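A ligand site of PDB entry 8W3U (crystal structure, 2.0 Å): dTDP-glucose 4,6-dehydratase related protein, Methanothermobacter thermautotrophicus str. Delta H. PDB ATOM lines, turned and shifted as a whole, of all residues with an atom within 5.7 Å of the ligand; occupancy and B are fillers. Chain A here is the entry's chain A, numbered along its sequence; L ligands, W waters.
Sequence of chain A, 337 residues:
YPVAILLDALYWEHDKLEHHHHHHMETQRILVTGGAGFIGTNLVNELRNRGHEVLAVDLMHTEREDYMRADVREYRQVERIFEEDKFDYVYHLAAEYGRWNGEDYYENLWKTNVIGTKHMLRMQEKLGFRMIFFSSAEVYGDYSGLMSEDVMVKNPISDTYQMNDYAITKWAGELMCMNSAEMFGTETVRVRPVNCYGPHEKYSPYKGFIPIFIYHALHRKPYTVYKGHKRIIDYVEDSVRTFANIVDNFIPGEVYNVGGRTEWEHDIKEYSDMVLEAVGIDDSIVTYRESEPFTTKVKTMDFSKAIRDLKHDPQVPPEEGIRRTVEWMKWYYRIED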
ATOM      1  N   TYR A  97     -25.907  19.204  20.789  1.00  0.00           N
ATOM      2  CA  TYR A  97     -24.467  19.281  20.855  1.00  0.00           C
ATOM      3  C   TYR A  97     -23.775  18.064  20.211  1.00  0.00           C
ATOM      4  O   TYR A  97     -24.153  16.935  20.466  1.00  0.00           O
ATOM      5  CB  TYR A  97     -24.022  19.422  22.317  1.00  0.00           C
ATOM      6  CG  TYR A  97     -22.555  19.156  22.520  1.00  0.00           C
ATOM      7  CD1 TYR A  97     -21.572  19.959  21.898  1.00  0.00           C
ATOM      8  CD2 TYR A  97     -22.137  18.086  23.329  1.00  0.00           C
ATOM      9  CE1 TYR A  97     -20.216  19.703  22.088  1.00  0.00           C
ATOM     10  CE2 TYR A  97     -20.785  17.817  23.517  1.00  0.00           C
ATOM     11  CZ  TYR A  97     -19.834  18.619  22.910  1.00  0.00           C
ATOM     12  OH  TYR A  97     -18.498  18.338  23.102  1.00  0.00           O
ATOM     13  N   ARG A  99     -20.731  16.747  16.942  1.00  0.00           N
ATOM     14  CA  ARG A  99     -20.694  16.467  15.517  1.00  0.00           C
ATOM     15  C   ARG A  99     -21.308  15.126  15.131  1.00  0.00           C
ATOM     16  O   ARG A  99     -22.090  15.071  14.179  1.00  0.00           O
ATOM     17  CB  ARG A  99     -19.291  16.640  14.951  1.00  0.00           C
ATOM     18  CG  ARG A  99     -18.199  15.829  15.641  1.00  0.00           C
ATOM     19  CD  ARG A  99     -16.842  16.441  15.356  1.00  0.00           C
ATOM     20  NE  ARG A  99     -15.794  15.746  16.091  1.00  0.00           N
ATOM     21  CZ  ARG A  99     -15.167  14.662  15.645  1.00  0.00           C
ATOM     22  NH1 ARG A  99     -15.453  14.165  14.447  1.00  0.00           N
ATOM     23  NH2 ARG A  99     -14.244  14.065  16.400  1.00  0.00           N
ATOM     24  N   GLU A 138     -15.786  24.663  16.162  1.00  0.00           N
ATOM     25  CA  GLU A 138     -15.930  23.890  14.916  1.00  0.00           C
ATOM     26  C   GLU A 138     -16.232  24.745  13.699  1.00  0.00           C
ATOM     27  O   GLU A 138     -16.062  24.282  12.568  1.00  0.00           O
ATOM     28  CB  GLU A 138     -16.941  22.757  15.038  1.00  0.00           C
ATOM     29  CG  GLU A 138     -16.565  21.742  16.114  1.00  0.00           C
ATOM     30  CD  GLU A 138     -17.006  20.352  15.779  1.00  0.00           C
ATOM     31  OE1 GLU A 138     -17.439  20.118  14.628  1.00  0.00           O
ATOM     32  OE2 GLU A 138     -16.925  19.488  16.664  1.00  0.00           O
ATOM     33  N   VAL A 194     -14.747  25.807  23.037  1.00  0.00           N
ATOM     34  CA  VAL A 194     -13.689  25.063  22.383  1.00  0.00           C
ATOM     35  C   VAL A 194     -13.823  23.570  22.686  1.00  0.00           C
ATOM     36  O   VAL A 194     -14.322  22.833  21.841  1.00  0.00           O
ATOM     37  CB  VAL A 194     -12.325  25.662  22.736  1.00  0.00           C
ATOM     38  CG1 VAL A 194     -11.194  24.911  22.056  1.00  0.00           C
ATOM     39  CG2 VAL A 194     -12.297  27.132  22.350  1.00  0.00           C
ATOM     40  N   ASN A 195     -13.366  23.134  23.853  1.00  0.00           N
ATOM     41  CA  ASN A 195     -13.285  21.692  24.206  1.00  0.00           C
ATOM     42  C   ASN A 195     -13.421  21.607  25.707  1.00  0.00           C
ATOM     43  O   ASN A 195     -12.487  21.291  26.450  1.00  0.00           O
ATOM     44  CB  ASN A 195     -11.944  21.041  23.731  1.00  0.00           C
ATOM     45  CG  ASN A 195     -11.904  20.792  22.210  1.00  0.00           C
ATOM     46  OD1 ASN A 195     -11.295  21.547  21.466  1.00  0.00           O
ATOM     47  ND2 ASN A 195     -12.555  19.710  21.759  1.00  0.00           N
ATOM     48  N   LYS A 207     -20.725  12.383  23.569  1.00  0.00           N
ATOM     49  CA  LYS A 207     -20.025  13.475  24.229  1.00  0.00           C
ATOM     50  C   LYS A 207     -18.667  13.618  23.561  1.00  0.00           C
ATOM     51  O   LYS A 207     -18.314  12.805  22.708  1.00  0.00           O
ATOM     52  CB  LYS A 207     -19.877  13.184  25.739  1.00  0.00           C
ATOM     53  CG  LYS A 207     -21.153  13.315  26.542  1.00  0.00           C
ATOM     54  CD  LYS A 207     -21.787  14.712  26.431  1.00  0.00           C
ATOM     55  CE  LYS A 207     -22.877  14.921  27.479  1.00  0.00           C
ATOM     56  NZ  LYS A 207     -23.534  16.269  27.387  1.00  0.00           N
ATOM     57  N   GLY A 208     -17.895  14.637  23.969  1.00  0.00           N
ATOM     58  CA  GLY A 208     -16.551  14.834  23.439  1.00  0.00           C
ATOM     59  C   GLY A 208     -15.572  13.826  24.031  1.00  0.00           C
ATOM     60  O   GLY A 208     -15.961  12.988  24.863  1.00  0.00           O
ATOM     61  N   PHE A 209     -14.325  13.894  23.589  1.00  0.00           N
ATOM     62  CA  PHE A 209     -13.334  12.864  23.893  1.00  0.00           C
ATOM     63  C   PHE A 209     -13.010  12.686  25.374  1.00  0.00           C
ATOM     64  O   PHE A 209     -12.840  11.556  25.802  1.00  0.00           O
ATOM     65  CB  PHE A 209     -12.079  13.035  23.053  1.00  0.00           C
ATOM     66  CG  PHE A 209     -11.123  14.167  23.464  1.00  0.00           C
ATOM     67  CD1 PHE A 209     -11.531  15.507  23.491  1.00  0.00           C
ATOM     68  CD2 PHE A 209      -9.770  13.881  23.704  1.00  0.00           C
ATOM     69  CE1 PHE A 209     -10.617  16.529  23.786  1.00  0.00           C
ATOM     70  CE2 PHE A 209      -8.856  14.887  24.005  1.00  0.00           C
ATOM     71  CZ  PHE A 209      -9.287  16.216  24.051  1.00  0.00           C
ATOM     72  N   ILE A 210     -12.967  13.787  26.124  1.00  0.00           N
ATOM     73  CA  ILE A 210     -12.585  13.732  27.535  1.00  0.00           C
ATOM     74  C   ILE A 210     -13.512  12.841  28.367  1.00  0.00           C
ATOM     75  O   ILE A 210     -13.033  11.887  28.964  1.00  0.00           O
ATOM     76  CB  ILE A 210     -12.302  15.122  28.164  1.00  0.00           C
ATOM     77  CG1 ILE A 210     -11.086  15.783  27.479  1.00  0.00           C
ATOM     78  CG2 ILE A 210     -12.128  15.020  29.660  1.00  0.00           C
ATOM     79  CD1 ILE A 210      -9.753  15.054  27.606  1.00  0.00           C
ATOM     80  N   ILE A 212     -15.544  10.606  27.312  1.00  0.00           N
ATOM     81  CA  ILE A 212     -15.460   9.247  26.734  1.00  0.00           C
ATOM     82  C   ILE A 212     -14.236   8.503  27.299  1.00  0.00           C
ATOM     83  O   ILE A 212     -14.360   7.374  27.800  1.00  0.00           O
ATOM     84  CB  ILE A 212     -15.434   9.306  25.174  1.00  0.00           C
ATOM     85  CG1 ILE A 212     -16.813   9.762  24.630  1.00  0.00           C
ATOM     86  CG2 ILE A 212     -14.991   7.974  24.558  1.00  0.00           C
ATOM     87  CD1 ILE A 212     -16.826  10.069  23.154  1.00  0.00           C
ATOM     88  N   PHE A 213     -13.079   9.158  27.262  1.00  0.00           N
ATOM     89  CA  PHE A 213     -11.839   8.578  27.801  1.00  0.00           C
ATOM     90  C   PHE A 213     -12.016   8.208  29.293  1.00  0.00           C
ATOM     91  O   PHE A 213     -11.748   7.082  29.675  1.00  0.00           O
ATOM     92  CB  PHE A 213     -10.676   9.555  27.651  1.00  0.00           C
ATOM     93  CG  PHE A 213     -10.158   9.720  26.244  1.00  0.00           C
ATOM     94  CD1 PHE A 213     -10.772   9.097  25.131  1.00  0.00           C
ATOM     95  CD2 PHE A 213      -9.048  10.546  26.017  1.00  0.00           C
ATOM     96  CE1 PHE A 213     -10.261   9.266  23.844  1.00  0.00           C
ATOM     97  CE2 PHE A 213      -8.555  10.742  24.734  1.00  0.00           C
ATOM     98  CZ  PHE A 213      -9.152  10.103  23.643  1.00  0.00           C
ATOM     99  N   TYR A 223     -11.209   1.926  24.530  1.00  0.00           N
ATOM    100  CA  TYR A 223     -11.578   3.144  23.776  1.00  0.00           C
ATOM    101  C   TYR A 223     -10.479   3.454  22.765  1.00  0.00           C
ATOM    102  O   TYR A 223      -9.369   2.930  22.877  1.00  0.00           O
ATOM    103  CB  TYR A 223     -11.836   4.339  24.722  1.00  0.00           C
ATOM    104  CG  TYR A 223     -10.644   4.856  25.524  1.00  0.00           C
ATOM    105  CD1 TYR A 223     -10.368   4.352  26.815  1.00  0.00           C
ATOM    106  CD2 TYR A 223      -9.826   5.869  25.022  1.00  0.00           C
ATOM    107  CE1 TYR A 223      -9.298   4.845  27.564  1.00  0.00           C
ATOM    108  CE2 TYR A 223      -8.756   6.362  25.772  1.00  0.00           C
ATOM    109  CZ  TYR A 223      -8.501   5.844  27.045  1.00  0.00           C
ATOM    110  OH  TYR A 223      -7.442   6.313  27.782  1.00  0.00           O
ATOM    111  N   THR A 224     -10.794   4.320  21.809  1.00  0.00           N
ATOM    112  CA  THR A 224      -9.900   4.635  20.703  1.00  0.00           C
ATOM    113  C   THR A 224      -9.287   6.031  20.854  1.00  0.00           C
ATOM    114  O   THR A 224      -9.976   6.975  21.218  1.00  0.00           O
ATOM    115  CB  THR A 224     -10.689   4.557  19.380  1.00  0.00           C
ATOM    116  OG1 THR A 224     -11.210   3.240  19.267  1.00  0.00           O
ATOM    117  CG2 THR A 224      -9.828   4.877  18.165  1.00  0.00           C
ATOM    118  N   VAL A 225      -7.992   6.126  20.569  1.00  0.00           N
ATOM    119  CA  VAL A 225      -7.291   7.396  20.535  1.00  0.00           C
ATOM    120  C   VAL A 225      -6.819   7.621  19.111  1.00  0.00           C
ATOM    121  O   VAL A 225      -6.013   6.816  18.571  1.00  0.00           O
ATOM    122  CB  VAL A 225      -6.088   7.407  21.500  1.00  0.00           C
ATOM    123  CG1 VAL A 225      -5.155   8.584  21.247  1.00  0.00           C
ATOM    124  CG2 VAL A 225      -6.594   7.397  22.938  1.00  0.00           C
ATOM    125  N   TYR A 226      -7.351   8.680  18.502  1.00  0.00           N
ATOM    126  CA  TYR A 226      -6.891   9.147  17.203  1.00  0.00           C
ATOM    127  C   TYR A 226      -5.721  10.070  17.447  1.00  0.00           C
ATOM    128  O   TYR A 226      -5.891  11.173  17.967  1.00  0.00           O
ATOM    129  CB  TYR A 226      -8.004   9.841  16.407  1.00  0.00           C
ATOM    130  CG  TYR A 226      -9.195   8.942  16.145  1.00  0.00           C
ATOM    131  CD1 TYR A 226      -9.165   7.971  15.123  1.00  0.00           C
ATOM    132  CD2 TYR A 226     -10.348   9.055  16.942  1.00  0.00           C
ATOM    133  CE1 TYR A 226     -10.235   7.117  14.920  1.00  0.00           C
ATOM    134  CE2 TYR A 226     -11.439   8.209  16.728  1.00  0.00           C
ATOM    135  CZ  TYR A 226     -11.372   7.258  15.706  1.00  0.00           C
ATOM    136  OH  TYR A 226     -12.451   6.436  15.506  1.00  0.00           O
ATOM    137  N   LYS A 227      -4.532   9.607  17.079  1.00  0.00           N
ATOM    138  CA  LYS A 227      -3.267  10.250  17.459  1.00  0.00           C
ATOM    139  C   LYS A 227      -3.008  11.612  16.814  1.00  0.00           C
ATOM    140  O   LYS A 227      -2.575  12.527  17.504  1.00  0.00           O
ATOM    141  CB  LYS A 227      -2.080   9.315  17.202  1.00  0.00           C
ATOM    142  CG  LYS A 227      -1.938   8.202  18.224  1.00  0.00           C
ATOM    143  CD  LYS A 227      -1.153   7.017  17.682  1.00  0.00           C
ATOM    144  CE  LYS A 227       0.364   7.241  17.675  1.00  0.00           C
ATOM    145  NZ  LYS A 227       1.012   6.231  16.804  1.00  0.00           N
ATOM    146  N   HIS A 229      -3.991  14.522  16.143  1.00  0.00           N
ATOM    147  CA  HIS A 229      -4.813  15.701  16.436  1.00  0.00           C
ATOM    148  C   HIS A 229      -4.295  16.386  17.683  1.00  0.00           C
ATOM    149  O   HIS A 229      -3.737  15.713  18.556  1.00  0.00           O
ATOM    150  CB  HIS A 229      -6.275  15.310  16.677  1.00  0.00           C
ATOM    151  CG  HIS A 229      -6.888  14.524  15.561  1.00  0.00           C
ATOM    152  ND1 HIS A 229      -7.607  15.103  14.541  1.00  0.00           N
ATOM    153  CD2 HIS A 229      -6.853  13.193  15.291  1.00  0.00           C
ATOM    154  CE1 HIS A 229      -8.002  14.166  13.700  1.00  0.00           C
ATOM    155  NE2 HIS A 229      -7.565  12.998  14.137  1.00  0.00           N
ATOM    156  N   LYS A 230      -4.461  17.715  17.739  1.00  0.00           N
ATOM    157  CA  LYS A 230      -4.146  18.510  18.933  1.00  0.00           C
ATOM    158  C   LYS A 230      -5.369  19.293  19.356  1.00  0.00           C
ATOM    159  O   LYS A 230      -6.154  19.770  18.521  1.00  0.00           O
ATOM    160  CB  LYS A 230      -2.983  19.467  18.685  1.00  0.00           C
ATOM    161  CG  LYS A 230      -1.685  18.790  18.303  1.00  0.00           C
ATOM    162  CD  LYS A 230      -0.614  19.830  18.022  1.00  0.00           C
ATOM    163  CE  LYS A 230       0.661  19.183  17.499  1.00  0.00           C
ATOM    164  NZ  LYS A 230       1.809  20.034  17.894  1.00  0.00           N
ATOM    165  N   ARG A 231      -5.557  19.404  20.665  1.00  0.00           N
ATOM    166  CA  ARG A 231      -6.648  20.179  21.230  1.00  0.00           C
ATOM    167  C   ARG A 231      -6.120  20.943  22.438  1.00  0.00           C
ATOM    168  O   ARG A 231      -5.098  20.542  23.055  1.00  0.00           O
ATOM    169  CB  ARG A 231      -7.783  19.240  21.676  1.00  0.00           C
ATOM    170  CG  ARG A 231      -8.566  18.548  20.544  1.00  0.00           C
ATOM    171  CD  ARG A 231      -9.232  19.577  19.635  1.00  0.00           C
ATOM    172  NE  ARG A 231     -10.025  18.948  18.584  1.00  0.00           N
ATOM    173  CZ  ARG A 231      -9.559  18.540  17.396  1.00  0.00           C
ATOM    174  NH1 ARG A 231      -8.274  18.683  17.061  1.00  0.00           N
ATOM    175  NH2 ARG A 231     -10.419  17.993  16.540  1.00  0.00           N
ATOM    176  N   ILE A 268      -3.679  14.020  21.329  1.00  0.00           N
ATOM    177  CA  ILE A 268      -4.761  13.257  21.965  1.00  0.00           C
ATOM    178  C   ILE A 268      -4.216  12.177  22.894  1.00  0.00           C
ATOM    179  O   ILE A 268      -4.790  11.928  23.969  1.00  0.00           O
ATOM    180  CB  ILE A 268      -5.736  12.677  20.924  1.00  0.00           C
ATOM    181  CG1 ILE A 268      -6.257  13.785  19.969  1.00  0.00           C
ATOM    182  CG2 ILE A 268      -6.879  11.925  21.593  1.00  0.00           C
ATOM    183  CD1 ILE A 268      -6.764  15.082  20.629  1.00  0.00           C
ATOM    184  N   GLU A 292      -8.459  10.655  12.892  1.00  0.00           N
ATOM    185  CA  GLU A 292      -9.884  10.491  12.654  1.00  0.00           C
ATOM    186  C   GLU A 292     -10.232  11.223  11.364  1.00  0.00           C
ATOM    187  O   GLU A 292      -9.921  12.418  11.219  1.00  0.00           O
ATOM    188  CB  GLU A 292     -10.734  11.025  13.812  1.00  0.00           C
ATOM    189  CG  GLU A 292     -12.143  10.477  13.842  1.00  0.00           C
ATOM    190  CD  GLU A 292     -13.048  11.203  14.831  1.00  0.00           C
ATOM    191  OE1 GLU A 292     -12.537  11.827  15.798  1.00  0.00           O
ATOM    192  OE2 GLU A 292     -14.278  11.182  14.623  1.00  0.00           O
ATOM    193  N   THR A 295     -12.124  15.167  10.754  1.00  0.00           N
ATOM    194  CA  THR A 295     -12.002  15.733  12.074  1.00  0.00           C
ATOM    195  C   THR A 295     -10.903  16.791  11.991  1.00  0.00           C
ATOM    196  O   THR A 295      -9.902  16.586  11.321  1.00  0.00           O
ATOM    197  CB  THR A 295     -11.652  14.609  13.049  1.00  0.00           C
ATOM    198  OG1 THR A 295     -12.738  13.660  13.044  1.00  0.00           O
ATOM    199  CG2 THR A 295     -11.419  15.143  14.468  1.00  0.00           C
ATOM    200  N   THR A 296     -11.111  17.931  12.655  1.00  0.00           N
ATOM    201  CA  THR A 296     -10.100  18.974  12.668  1.00  0.00           C
ATOM    202  C   THR A 296      -8.779  18.428  13.224  1.00  0.00           C
ATOM    203  O   THR A 296      -8.766  17.804  14.294  1.00  0.00           O
ATOM    204  CB  THR A 296     -10.591  20.166  13.484  1.00  0.00           C
ATOM    205  OG1 THR A 296     -11.764  20.685  12.848  1.00  0.00           O
ATOM    206  CG2 THR A 296      -9.532  21.253  13.602  1.00  0.00           C
ATOM    207  N   LYS A 297      -7.702  18.665  12.501  1.00  0.00           N
ATOM    208  CA  LYS A 297      -6.391  18.168  12.870  1.00  0.00           C
ATOM    209  C   LYS A 297      -5.872  18.937  14.106  1.00  0.00           C
ATOM    210  O   LYS A 297      -5.557  18.332  15.140  1.00  0.00           O
ATOM    211  CB  LYS A 297      -5.441  18.240  11.663  1.00  0.00           C
ATOM    212  CG  LYS A 297      -4.006  17.794  11.929  1.00  0.00           C
ATOM    213  CD  LYS A 297      -3.229  17.511  10.641  1.00  0.00           C
ATOM    214  CE  LYS A 297      -1.916  16.767  10.888  1.00  0.00           C
ATOM    215  NZ  LYS A 297      -1.140  17.300  12.044  1.00  0.00           N
ATOM    216  N   LYS A 299      -6.410  22.575  16.559  1.00  0.00           N
ATOM    217  CA  LYS A 299      -7.363  23.596  16.936  1.00  0.00           C
ATOM    218  C   LYS A 299      -6.659  24.596  17.831  1.00  0.00           C
ATOM    219  O   LYS A 299      -6.956  24.696  19.029  1.00  0.00           O
ATOM    220  CB  LYS A 299      -8.496  22.906  17.664  1.00  0.00           C
ATOM    221  CG  LYS A 299      -9.872  23.416  17.366  1.00  0.00           C
ATOM    222  CD  LYS A 299     -10.868  22.319  17.686  1.00  0.00           C
ATOM    223  CE  LYS A 299     -12.183  22.913  18.108  1.00  0.00           C
ATOM    224  NZ  LYS A 299     -13.263  21.886  18.110  1.00  0.00           N
HETATM  225  N1  LIG L   1     -11.206  11.537  19.844  1.00  0.00           N
HETATM  226  C1  LIG L   1     -10.554  10.359  20.127  1.00  0.00           C
HETATM  227  N2  LIG L   1     -11.351   9.350  20.575  1.00  0.00           N
HETATM  228  C2  LIG L   1     -12.716   9.393  20.773  1.00  0.00           C
HETATM  229  C3  LIG L   1     -13.330  10.642  20.446  1.00  0.00           C
HETATM  230  C4  LIG L   1     -12.569  11.648  19.993  1.00  0.00           C
HETATM  231  O1  LIG L   1      -9.341  10.220  19.996  1.00  0.00           O
HETATM  232  O2  LIG L   1     -13.294   8.396  21.187  1.00  0.00           O
HETATM  233  C5  LIG L   1     -10.400  12.657  19.345  1.00  0.00           C
HETATM  234  C6  LIG L   1     -10.905  13.186  18.012  1.00  0.00           C
HETATM  235  O3  LIG L   1     -10.289  12.434  16.992  1.00  0.00           O
HETATM  236  C7  LIG L   1     -10.442  14.649  18.059  1.00  0.00           C
HETATM  237  C8  LIG L   1     -10.456  14.998  19.563  1.00  0.00           C
HETATM  238  O4  LIG L   1     -10.502  13.726  20.259  1.00  0.00           O
HETATM  239  O5  LIG L   1      -9.142  14.821  17.530  1.00  0.00           O
HETATM  240  C9  LIG L   1     -11.604  15.861  20.009  1.00  0.00           C
HETATM  241  O6  LIG L   1     -12.813  15.384  19.389  1.00  0.00           O
HETATM  242  P1  LIG L   1     -14.232  15.910  19.898  1.00  0.00           P
HETATM  243  O7  LIG L   1     -14.319  15.690  21.369  1.00  0.00           O
HETATM  244  O8  LIG L   1     -15.284  15.344  19.025  1.00  0.00           O
HETATM  245  O9  LIG L   1     -14.096  17.480  19.663  1.00  0.00           O
HETATM  246  P2  LIG L   1     -13.690  18.431  18.444  1.00  0.00           P
HETATM  247  O10 LIG L   1     -12.566  19.270  18.950  1.00  0.00           O
HETATM  248  O11 LIG L   1     -13.308  17.566  17.285  1.00  0.00           O
HETATM  249  O12 LIG L   1     -14.876  19.254  18.183  1.00  0.00           O
HETATM  250  O   HOH W   1     -13.415  18.401  14.517  1.00  0.00           O
HETATM  251  O   HOH W   2     -16.067   8.156  20.299  1.00  0.00           O
HETATM  252  O   HOH W   3     -14.119  17.904  23.185  1.00  0.00           O
HETATM  253  O   HOH W   4     -13.298   5.693  21.660  1.00  0.00           O
HETATM  254  O   HOH W   5     -16.134  20.299  20.221  1.00  0.00           O
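The side-chain carboxylate (OE2) of Glu 138 sits close to an oxygen (O12) of the ligand. NE of Arg 231 lies within salt-bridge range of O10 of the ligand (2.6 Å). OE1 of Glu 292 sits at hydrogen-bond distance from O3 of the ligand (2.6 Å). The backbone carbonyl oxygen of Thr 224 sits at hydrogen-bond distance from a nitrogen (N2) of the ligand, 2.8 Å away. The side-chain amino group of Lys 299 is in salt-bridge range of an oxygen (O10) of the ligand (2.8 Å). ND2 of Asn 195 sits at hydrogen-bond distance from O10 of the ligand (2.8 Å). An oxygen (O7) of the ligand sits at hydrogen-bond distance from the backbone NH of Phe 209 (2.9 Å). N of Tyr 226 is in hydrogen-bond range of O1 of the ligand (2.9 Å). The guanidinium group (NE) of Arg 99 lies within salt-bridge range of an oxygen (O8) of the ligand (3.0 Å). An oxygen (O5) of the ligand lies close to a ring nitrogen (ND1) of His 229 (3.4 Å).
Residues that only touch the ligand: Gly 208 (3.2 Å), Ile 268 (3.4 Å), Phe 213 (3.4 Å), Val 225 (3.5 Å), Thr 295 (3.8 Å) and Ile 212 (3.8 Å). Hydrophobic or aromatic side chains that line the ligand: Phe 209, Ile 212, Phe 213, Tyr 226, His 229 and Ile 268. 16 residues have an atom within 4 Å of the ligand: Arg 99, Glu 138, Asn 195, Gly 208, Phe 209, Ile 212, Phe 213, Thr 224, Val 225, Tyr 226, His 229, Arg 231, Ile 268, Glu 292, Thr 295 and Lys 299. The nearest printed residue that does not touch the ligand is Thr 296 (4.4 Å).
The guanidinium group of Arg 231 lies within hydrogen-bond range of the backbone carbonyl oxygen of Thr 296 (2.8 Å). The backbone carbonyl oxygen (O) of Lys 297 lies within hydrogen-bond range of the guanidinium group (NH1) of Arg 231, 3.3 Å away. The backbone NH (N) of Glu 292 sits at hydrogen-bond distance from a ring nitrogen (NE2) of His 229, at 2.8 Å. The side-chain carboxylate of Glu 292 lies close to the side-chain hydroxyl of Thr 295 (3.3 Å). N of Lys 299 lies within hydrogen-bond range of O of Lys 230 (3.4 Å). The side-chain hydroxyl (OG1) of Thr 295 sits at hydrogen-bond distance from the guanidinium group (NH1) of Arg 99 (3.1 Å). O of His 229 sits at hydrogen-bond distance from N of Ile 268, at 3.2 Å. A ring nitrogen (ND1) of His 229 sits at hydrogen-bond distance from the backbone carbonyl oxygen of Thr 296 (2.9 Å).
Water W4 bridges an oxygen (O2) of the ligand and the backbone NH (N) of Thr 224. Water W3 bridges the side-chain amide nitrogen of Asn 195 (2.8 Å) and an oxygen (O7) of the ligand (2.9 Å). Water W1 bridges O11 of the ligand (2.9 Å) and N of Thr 296 (3.0 Å).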
